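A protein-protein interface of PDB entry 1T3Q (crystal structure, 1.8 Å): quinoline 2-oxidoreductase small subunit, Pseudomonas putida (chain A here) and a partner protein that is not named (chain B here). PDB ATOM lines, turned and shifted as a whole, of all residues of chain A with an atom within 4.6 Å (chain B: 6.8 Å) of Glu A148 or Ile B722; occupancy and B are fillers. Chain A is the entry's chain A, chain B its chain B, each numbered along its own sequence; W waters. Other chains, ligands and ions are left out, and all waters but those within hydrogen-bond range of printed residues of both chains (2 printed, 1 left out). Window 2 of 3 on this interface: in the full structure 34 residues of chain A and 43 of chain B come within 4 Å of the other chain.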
ATOM      1  N   ARG A 130      -3.724 -29.902  16.878  1.00  0.00           N
ATOM      2  CA  ARG A 130      -3.572 -28.900  15.831  1.00  0.00           C
ATOM      3  C   ARG A 130      -3.763 -27.507  16.430  1.00  0.00           C
ATOM      4  O   ARG A 130      -3.038 -26.575  16.086  1.00  0.00           O
ATOM      5  CB  ARG A 130      -4.584 -29.141  14.703  1.00  0.00           C
ATOM      6  CG  ARG A 130      -4.327 -30.412  13.906  1.00  0.00           C
ATOM      7  CD  ARG A 130      -5.325 -30.571  12.763  1.00  0.00           C
ATOM      8  NE  ARG A 130      -5.130 -29.564  11.722  1.00  0.00           N
ATOM      9  CZ  ARG A 130      -4.228 -29.652  10.751  1.00  0.00           C
ATOM     10  NH1 ARG A 130      -3.433 -30.712  10.677  1.00  0.00           N
ATOM     11  NH2 ARG A 130      -4.115 -28.678   9.856  1.00  0.00           N
ATOM     12  N   ARG A 134      -1.148 -24.389  16.324  1.00  0.00           N
ATOM     13  CA  ARG A 134      -1.490 -23.088  15.756  1.00  0.00           C
ATOM     14  C   ARG A 134      -1.262 -21.977  16.780  1.00  0.00           C
ATOM     15  O   ARG A 134      -0.820 -20.883  16.432  1.00  0.00           O
ATOM     16  CB  ARG A 134      -2.942 -23.074  15.265  1.00  0.00           C
ATOM     17  CG  ARG A 134      -3.143 -23.792  13.922  1.00  0.00           C
ATOM     18  CD  ARG A 134      -4.607 -23.792  13.494  1.00  0.00           C
ATOM     19  NE  ARG A 134      -4.832 -24.467  12.214  1.00  0.00           N
ATOM     20  CZ  ARG A 134      -4.591 -23.927  11.021  1.00  0.00           C
ATOM     21  NH1 ARG A 134      -4.111 -22.695  10.931  1.00  0.00           N
ATOM     22  NH2 ARG A 134      -4.841 -24.615   9.917  1.00  0.00           N
ATOM     23  N   GLY A 146      -0.025 -20.410   3.816  1.00  0.00           N
ATOM     24  CA  GLY A 146      -1.372 -20.472   4.350  1.00  0.00           C
ATOM     25  C   GLY A 146      -1.396 -21.296   5.635  1.00  0.00           C
ATOM     26  O   GLY A 146      -2.459 -21.607   6.162  1.00  0.00           O
ATOM     27  N   TYR A 147      -0.211 -21.677   6.107  1.00  0.00           N
ATOM     28  CA  TYR A 147      -0.022 -22.414   7.366  1.00  0.00           C
ATOM     29  C   TYR A 147      -0.541 -23.835   7.552  1.00  0.00           C
ATOM     30  O   TYR A 147       0.043 -24.592   8.331  1.00  0.00           O
ATOM     31  CB  TYR A 147      -0.577 -21.601   8.533  1.00  0.00           C
ATOM     32  CG  TYR A 147       0.023 -20.227   8.687  1.00  0.00           C
ATOM     33  CD1 TYR A 147       1.330 -20.061   9.134  1.00  0.00           C
ATOM     34  CD2 TYR A 147      -0.728 -19.092   8.399  1.00  0.00           C
ATOM     35  CE1 TYR A 147       1.879 -18.785   9.296  1.00  0.00           C
ATOM     36  CE2 TYR A 147      -0.193 -17.815   8.557  1.00  0.00           C
ATOM     37  CZ  TYR A 147       1.105 -17.670   9.007  1.00  0.00           C
ATOM     38  OH  TYR A 147       1.618 -16.408   9.187  1.00  0.00           O
ATOM     39  N   GLU A 148      -1.625 -24.206   6.881  1.00  0.00           N
ATOM     40  CA  GLU A 148      -2.177 -25.539   7.101  1.00  0.00           C
ATOM     41  C   GLU A 148      -1.185 -26.692   7.005  1.00  0.00           C
ATOM     42  O   GLU A 148      -1.179 -27.576   7.864  1.00  0.00           O
ATOM     43  CB  GLU A 148      -3.362 -25.818   6.169  1.00  0.00           C
ATOM     44  CG  GLU A 148      -3.989 -27.183   6.451  1.00  0.00           C
ATOM     45  CD  GLU A 148      -5.272 -27.435   5.694  1.00  0.00           C
ATOM     46  OE1 GLU A 148      -5.753 -28.589   5.729  1.00  0.00           O
ATOM     47  OE2 GLU A 148      -5.804 -26.490   5.075  1.00  0.00           O
ATOM     48  N   THR A 149      -0.331 -26.681   5.986  1.00  0.00           N
ATOM     49  CA  THR A 149       0.620 -27.768   5.818  1.00  0.00           C
ATOM     50  C   THR A 149       1.741 -27.788   6.857  1.00  0.00           C
ATOM     51  O   THR A 149       2.367 -28.824   7.069  1.00  0.00           O
ATOM     52  CB  THR A 149       1.216 -27.772   4.392  1.00  0.00           C
ATOM     53  OG1 THR A 149       1.698 -26.464   4.061  1.00  0.00           O
ATOM     54  CG2 THR A 149       0.147 -28.189   3.380  1.00  0.00           C
ATOM     55  N   ILE A 150       2.007 -26.648   7.487  1.00  0.00           N
ATOM     56  CA  ILE A 150       3.026 -26.596   8.530  1.00  0.00           C
ATOM     57  C   ILE A 150       2.421 -27.291   9.756  1.00  0.00           C
ATOM     58  O   ILE A 150       3.112 -28.028  10.475  1.00  0.00           O
ATOM     59  CB  ILE A 150       3.404 -25.135   8.888  1.00  0.00           C
ATOM     60  CG1 ILE A 150       4.169 -24.501   7.725  1.00  0.00           C
ATOM     61  CG2 ILE A 150       4.256 -25.104  10.150  1.00  0.00           C
ATOM     62  CD1 ILE A 150       4.439 -23.012   7.895  1.00  0.00           C
ATOM     63  N   ILE A 151       1.128 -27.063   9.980  1.00  0.00           N
ATOM     64  CA  ILE A 151       0.433 -27.690  11.105  1.00  0.00           C
ATOM     65  C   ILE A 151       0.423 -29.197  10.832  1.00  0.00           C
ATOM     66  O   ILE A 151       0.653 -30.007  11.735  1.00  0.00           O
ATOM     67  CB  ILE A 151      -1.027 -27.186  11.235  1.00  0.00           C
ATOM     68  CG1 ILE A 151      -1.057 -25.656  11.317  1.00  0.00           C
ATOM     69  CG2 ILE A 151      -1.687 -27.782  12.480  1.00  0.00           C
ATOM     70  CD1 ILE A 151      -0.273 -25.064  12.474  1.00  0.00           C
ATOM     71  N   ASP A 152       0.166 -29.564   9.580  1.00  0.00           N
ATOM     72  CA  ASP A 152       0.147 -30.971   9.179  1.00  0.00           C
ATOM     73  C   ASP A 152       1.501 -31.622   9.455  1.00  0.00           C
ATOM     74  O   ASP A 152       1.572 -32.723   9.998  1.00  0.00           O
ATOM     75  CB  ASP A 152      -0.134 -31.112   7.678  1.00  0.00           C
ATOM     76  CG  ASP A 152      -1.529 -30.664   7.284  1.00  0.00           C
ATOM     77  OD1 ASP A 152      -1.761 -30.522   6.064  1.00  0.00           O
ATOM     78  OD2 ASP A 152      -2.390 -30.469   8.167  1.00  0.00           O
ATOM     79  N   ASP B 659     -14.366 -21.248   7.896  1.00  0.00           N
ATOM     80  CA  ASP B 659     -14.301 -22.234   6.828  1.00  0.00           C
ATOM     81  C   ASP B 659     -13.929 -21.596   5.496  1.00  0.00           C
ATOM     82  O   ASP B 659     -14.221 -20.430   5.248  1.00  0.00           O
ATOM     83  CB  ASP B 659     -15.659 -22.919   6.653  1.00  0.00           C
ATOM     84  CG  ASP B 659     -16.146 -23.589   7.918  1.00  0.00           C
ATOM     85  OD1 ASP B 659     -15.847 -24.785   8.113  1.00  0.00           O
ATOM     86  OD2 ASP B 659     -16.829 -22.918   8.715  1.00  0.00           O
ATOM     87  N   PHE B 660     -13.286 -22.378   4.643  1.00  0.00           N
ATOM     88  CA  PHE B 660     -12.923 -21.908   3.318  1.00  0.00           C
ATOM     89  C   PHE B 660     -12.966 -23.093   2.372  1.00  0.00           C
ATOM     90  O   PHE B 660     -12.398 -24.156   2.649  1.00  0.00           O
ATOM     91  CB  PHE B 660     -11.538 -21.257   3.320  1.00  0.00           C
ATOM     92  CG  PHE B 660     -11.512 -19.917   2.638  1.00  0.00           C
ATOM     93  CD1 PHE B 660     -11.692 -19.817   1.262  1.00  0.00           C
ATOM     94  CD2 PHE B 660     -11.362 -18.749   3.380  1.00  0.00           C
ATOM     95  CE1 PHE B 660     -11.731 -18.570   0.634  1.00  0.00           C
ATOM     96  CE2 PHE B 660     -11.397 -17.499   2.762  1.00  0.00           C
ATOM     97  CZ  PHE B 660     -11.583 -17.409   1.387  1.00  0.00           C
ATOM     98  N   PHE B 661     -13.677 -22.905   1.270  1.00  0.00           N
ATOM     99  CA  PHE B 661     -13.842 -23.936   0.261  1.00  0.00           C
ATOM    100  C   PHE B 661     -13.322 -23.388  -1.058  1.00  0.00           C
ATOM    101  O   PHE B 661     -13.588 -22.237  -1.402  1.00  0.00           O
ATOM    102  CB  PHE B 661     -15.322 -24.281   0.124  1.00  0.00           C
ATOM    103  CG  PHE B 661     -15.991 -24.627   1.430  1.00  0.00           C
ATOM    104  CD1 PHE B 661     -15.928 -25.920   1.943  1.00  0.00           C
ATOM    105  CD2 PHE B 661     -16.684 -23.658   2.146  1.00  0.00           C
ATOM    106  CE1 PHE B 661     -16.552 -26.238   3.152  1.00  0.00           C
ATOM    107  CE2 PHE B 661     -17.309 -23.968   3.354  1.00  0.00           C
ATOM    108  CZ  PHE B 661     -17.242 -25.258   3.856  1.00  0.00           C
ATOM    109  N   ALA B 662     -12.579 -24.208  -1.792  1.00  0.00           N
ATOM    110  CA  ALA B 662     -12.033 -23.781  -3.070  1.00  0.00           C
ATOM    111  C   ALA B 662     -12.211 -24.823  -4.163  1.00  0.00           C
ATOM    112  O   ALA B 662     -12.014 -26.018  -3.939  1.00  0.00           O
ATOM    113  CB  ALA B 662     -10.546 -23.448  -2.919  1.00  0.00           C
ATOM    114  N   GLU B 676      -2.053 -26.928  -4.697  1.00  0.00           N
ATOM    115  CA  GLU B 676      -2.839 -26.680  -3.498  1.00  0.00           C
ATOM    116  C   GLU B 676      -2.095 -25.739  -2.566  1.00  0.00           C
ATOM    117  O   GLU B 676      -2.716 -24.951  -1.863  1.00  0.00           O
ATOM    118  CB  GLU B 676      -3.203 -27.989  -2.785  1.00  0.00           C
ATOM    119  CG  GLU B 676      -4.224 -28.819  -3.568  1.00  0.00           C
ATOM    120  CD  GLU B 676      -4.980 -29.818  -2.707  1.00  0.00           C
ATOM    121  OE1 GLU B 676      -4.673 -29.932  -1.500  1.00  0.00           O
ATOM    122  OE2 GLU B 676      -5.891 -30.486  -3.242  1.00  0.00           O
ATOM    123  N   ILE B 679      -2.896 -22.370  -3.728  1.00  0.00           N
ATOM    124  CA  ILE B 679      -4.260 -22.001  -3.381  1.00  0.00           C
ATOM    125  C   ILE B 679      -4.357 -21.579  -1.914  1.00  0.00           C
ATOM    126  O   ILE B 679      -4.969 -20.558  -1.593  1.00  0.00           O
ATOM    127  CB  ILE B 679      -5.241 -23.177  -3.636  1.00  0.00           C
ATOM    128  CG1 ILE B 679      -5.413 -23.398  -5.141  1.00  0.00           C
ATOM    129  CG2 ILE B 679      -6.583 -22.885  -2.987  1.00  0.00           C
ATOM    130  CD1 ILE B 679      -6.170 -24.675  -5.490  1.00  0.00           C
ATOM    131  N   ARG B 680      -3.766 -22.363  -1.015  1.00  0.00           N
ATOM    132  CA  ARG B 680      -3.819 -22.021   0.403  1.00  0.00           C
ATOM    133  C   ARG B 680      -3.057 -20.731   0.690  1.00  0.00           C
ATOM    134  O   ARG B 680      -3.510 -19.900   1.473  1.00  0.00           O
ATOM    135  CB  ARG B 680      -3.273 -23.178   1.257  1.00  0.00           C
ATOM    136  CG  ARG B 680      -4.152 -24.424   1.187  1.00  0.00           C
ATOM    137  CD  ARG B 680      -3.871 -25.399   2.332  1.00  0.00           C
ATOM    138  NE  ARG B 680      -4.894 -26.446   2.392  1.00  0.00           N
ATOM    139  CZ  ARG B 680      -4.912 -27.530   1.622  1.00  0.00           C
ATOM    140  NH1 ARG B 680      -5.895 -28.412   1.755  1.00  0.00           N
ATOM    141  NH2 ARG B 680      -3.943 -27.747   0.737  1.00  0.00           N
ATOM    142  N   GLY B 681      -1.911 -20.556   0.044  1.00  0.00           N
ATOM    143  CA  GLY B 681      -1.135 -19.342   0.255  1.00  0.00           C
ATOM    144  C   GLY B 681      -1.909 -18.115  -0.191  1.00  0.00           C
ATOM    145  O   GLY B 681      -1.919 -17.089   0.497  1.00  0.00           O
ATOM    146  N   ILE B 683      -5.163 -17.847  -0.443  1.00  0.00           N
ATOM    147  CA  ILE B 683      -6.307 -17.660   0.440  1.00  0.00           C
ATOM    148  C   ILE B 683      -5.914 -16.918   1.718  1.00  0.00           C
ATOM    149  O   ILE B 683      -6.667 -16.073   2.207  1.00  0.00           O
ATOM    150  CB  ILE B 683      -6.969 -19.021   0.806  1.00  0.00           C
ATOM    151  CG1 ILE B 683      -7.742 -19.553  -0.411  1.00  0.00           C
ATOM    152  CG2 ILE B 683      -7.920 -18.843   2.006  1.00  0.00           C
ATOM    153  CD1 ILE B 683      -8.278 -20.975  -0.254  1.00  0.00           C
ATOM    154  N   ALA B 684      -4.740 -17.224   2.260  1.00  0.00           N
ATOM    155  CA  ALA B 684      -4.285 -16.549   3.472  1.00  0.00           C
ATOM    156  C   ALA B 684      -4.083 -15.056   3.187  1.00  0.00           C
ATOM    157  O   ALA B 684      -4.506 -14.201   3.967  1.00  0.00           O
ATOM    158  CB  ALA B 684      -2.985 -17.176   3.978  1.00  0.00           C
ATOM    159  N   ILE B 687      -7.382 -13.300   3.086  1.00  0.00           N
ATOM    160  CA  ILE B 687      -7.944 -13.041   4.401  1.00  0.00           C
ATOM    161  C   ILE B 687      -7.225 -11.821   4.980  1.00  0.00           C
ATOM    162  O   ILE B 687      -7.827 -10.990   5.666  1.00  0.00           O
ATOM    163  CB  ILE B 687      -7.748 -14.265   5.316  1.00  0.00           C
ATOM    164  CG1 ILE B 687      -8.699 -15.377   4.868  1.00  0.00           C
ATOM    165  CG2 ILE B 687      -7.976 -13.882   6.778  1.00  0.00           C
ATOM    166  CD1 ILE B 687      -8.388 -16.746   5.474  1.00  0.00           C
ATOM    167  N   THR B 716      -1.176 -18.138  12.030  1.00  0.00           N
ATOM    168  CA  THR B 716      -1.787 -19.461  12.108  1.00  0.00           C
ATOM    169  C   THR B 716      -3.185 -19.391  12.730  1.00  0.00           C
ATOM    170  O   THR B 716      -3.990 -20.310  12.572  1.00  0.00           O
ATOM    171  CB  THR B 716      -0.939 -20.395  12.989  1.00  0.00           C
ATOM    172  OG1 THR B 716      -0.607 -19.708  14.200  1.00  0.00           O
ATOM    173  CG2 THR B 716       0.334 -20.815  12.277  1.00  0.00           C
ATOM    174  N   VAL B 719      -6.007 -18.081   9.639  1.00  0.00           N
ATOM    175  CA  VAL B 719      -6.363 -18.927   8.508  1.00  0.00           C
ATOM    176  C   VAL B 719      -6.856 -20.290   8.970  1.00  0.00           C
ATOM    177  O   VAL B 719      -6.163 -20.998   9.706  1.00  0.00           O
ATOM    178  CB  VAL B 719      -5.149 -19.121   7.566  1.00  0.00           C
ATOM    179  CG1 VAL B 719      -5.603 -19.710   6.232  1.00  0.00           C
ATOM    180  CG2 VAL B 719      -4.438 -17.787   7.354  1.00  0.00           C
ATOM    181  N   PRO B 720      -8.066 -20.678   8.540  1.00  0.00           N
ATOM    182  CA  PRO B 720      -8.638 -21.971   8.926  1.00  0.00           C
ATOM    183  C   PRO B 720      -8.091 -23.069   8.033  1.00  0.00           C
ATOM    184  O   PRO B 720      -7.310 -22.805   7.116  1.00  0.00           O
ATOM    185  CB  PRO B 720     -10.124 -21.759   8.687  1.00  0.00           C
ATOM    186  CG  PRO B 720     -10.102 -20.947   7.401  1.00  0.00           C
ATOM    187  CD  PRO B 720      -9.002 -19.925   7.681  1.00  0.00           C
ATOM    188  N   ASP B 721      -8.479 -24.310   8.304  1.00  0.00           N
ATOM    189  CA  ASP B 721      -8.060 -25.392   7.429  1.00  0.00           C
ATOM    190  C   ASP B 721      -8.914 -25.132   6.190  1.00  0.00           C
ATOM    191  O   ASP B 721     -10.034 -24.632   6.299  1.00  0.00           O
ATOM    192  CB  ASP B 721      -8.367 -26.756   8.046  1.00  0.00           C
ATOM    193  CG  ASP B 721      -7.458 -27.069   9.222  1.00  0.00           C
ATOM    194  OD1 ASP B 721      -6.226 -26.926   9.072  1.00  0.00           O
ATOM    195  OD2 ASP B 721      -7.966 -27.454  10.294  1.00  0.00           O
ATOM    196  N   ILE B 722      -8.377 -25.460   5.024  1.00  0.00           N
ATOM    197  CA  ILE B 722      -9.050 -25.204   3.758  1.00  0.00           C
ATOM    198  C   ILE B 722      -9.372 -26.473   2.976  1.00  0.00           C
ATOM    199  O   ILE B 722      -8.532 -27.368   2.864  1.00  0.00           O
ATOM    200  CB  ILE B 722      -8.145 -24.286   2.893  1.00  0.00           C
ATOM    201  CG1 ILE B 722      -7.939 -22.956   3.621  1.00  0.00           C
ATOM    202  CG2 ILE B 722      -8.745 -24.084   1.506  1.00  0.00           C
ATOM    203  CD1 ILE B 722      -6.671 -22.214   3.207  1.00  0.00           C
ATOM    204  N   ARG B 723     -10.588 -26.549   2.437  1.00  0.00           N
ATOM    205  CA  ARG B 723     -10.987 -27.709   1.642  1.00  0.00           C
ATOM    206  C   ARG B 723     -10.907 -27.344   0.162  1.00  0.00           C
ATOM    207  O   ARG B 723     -11.459 -26.332  -0.276  1.00  0.00           O
ATOM    208  CB  ARG B 723     -12.404 -28.167   2.002  1.00  0.00           C
ATOM    209  CG  ARG B 723     -12.769 -29.537   1.421  1.00  0.00           C
ATOM    210  CD  ARG B 723     -13.790 -30.266   2.296  1.00  0.00           C
ATOM    211  NE  ARG B 723     -15.149 -30.262   1.755  1.00  0.00           N
ATOM    212  CZ  ARG B 723     -15.556 -31.009   0.731  1.00  0.00           C
ATOM    213  NH1 ARG B 723     -16.814 -30.940   0.314  1.00  0.00           N
ATOM    214  NH2 ARG B 723     -14.711 -31.820   0.119  1.00  0.00           N
ATOM    215  N   ILE B 724     -10.207 -28.175  -0.603  1.00  0.00           N
ATOM    216  CA  ILE B 724     -10.017 -27.926  -2.027  1.00  0.00           C
ATOM    217  C   ILE B 724     -10.464 -29.068  -2.921  1.00  0.00           C
ATOM    218  O   ILE B 724     -10.208 -30.228  -2.626  1.00  0.00           O
ATOM    219  CB  ILE B 724      -8.528 -27.696  -2.345  1.00  0.00           C
ATOM    220  CG1 ILE B 724      -7.980 -26.545  -1.502  1.00  0.00           C
ATOM    221  CG2 ILE B 724      -8.345 -27.435  -3.838  1.00  0.00           C
ATOM    222  CD1 ILE B 724      -6.470 -26.380  -1.625  1.00  0.00           C
HETATM  223  O   HOH W   1      -8.097 -29.201   4.771  1.00  0.00           O
HETATM  224  O   HOH W   2      -6.247 -26.749  12.325  1.00  0.00           O
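The guanidinium group (NH2) of Arg A130 lies within salt-bridge range of the side-chain carboxylate (OD1) of Asp B721 (2.9 Å).
The backbone carbonyl oxygen (O) of Arg A134 lies within hydrogen-bond range of the side-chain hydroxyl (OG1) of Thr B716 (2.5 Å).
NH1 of Arg A134 lies within hydrogen-bond range of O of Val B719, 2.9 Å away.
The guanidinium group (NH2) of Arg A134 lies within salt-bridge range of the side-chain carboxylate (OD1) of Asp B721.
NE of Arg B680 is in salt-bridge range of OE2 of Glu A148 (2.8 Å).
The backbone NH (N) of Ile B722 lies within hydrogen-bond range of the side-chain carboxylate (OE2) of Glu A148 (2.8 Å).
NH1 of Arg A130 is in salt-bridge range of OD2 of Asp A152 (2.7 Å).
The side-chain carboxylate of Glu B676 lies within salt-bridge range of the guanidinium group of Arg B680, at 3.2 Å.
The backbone carbonyl oxygen (O) of Ile B722 sits at hydrogen-bond distance from the guanidinium group (NH1) of Arg B680, 3.0 Å away.
Gly A146 touches Arg B680.
Gly B681 touches Gly A146 (CA to N, 3.9 Å).
Ala B684 touches Gly A146 (CB to CA, 3.7 Å).
Gly A146 touches Val B719 (O to CG1, 3.7 Å).
Thr B716 touches Tyr A147 (CG2 to CD1, 3.4 Å).
CA of Asp B721 touches OE2 of Glu A148 (3.4 Å).
Of the printed residues of chain B, Arg A134 touches Thr B716 (2.5 Å), Val B719 (2.9 Å) and Asp B721 (2.8 Å).
Printed residues of chain B within 4 Å of Tyr A147: Thr B716 (3.4 Å).
Glu A148 touches just these residues of chain B: Arg B680 (2.8 Å), Asp B721 (3.4 Å) and Ile B722 (2.8 Å).
Of the printed residues of chain A, Gly B681 touches Gly A146.
Printed residues of chain A within 4 Å of Ala B684: Gly A146.
Printed residues of chain A within 4 Å of Val B719: Arg A134 (2.9 Å) and Gly A146 (3.7 Å).
Ile B722 touches one residue of chain A.
The nearest residue of chain B that does not touch Glu A148 is Pro B720 (4.5 Å).
Printed residues of chain B that touch a printed residue of chain A: Arg B680, Gly B681, Ala B684, Thr B716, Val B719, Asp B721 and Ile B722.
Hydrophobic or aromatic side chains of chain B that line the printed part of chain A: Ala B684, Val B719 and Ile B722.
Among the printed residues, 12 pairs touch across the chains.
Water W1 bridges the side-chain carboxylate of Glu A148 (2.6 Å) and the backbone carbonyl oxygen of Ile B722 (2.7 Å).
Water W2 lies within hydrogen-bond range of NE of Arg A134, OD2 of Asp B721 and NE of Arg A130.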
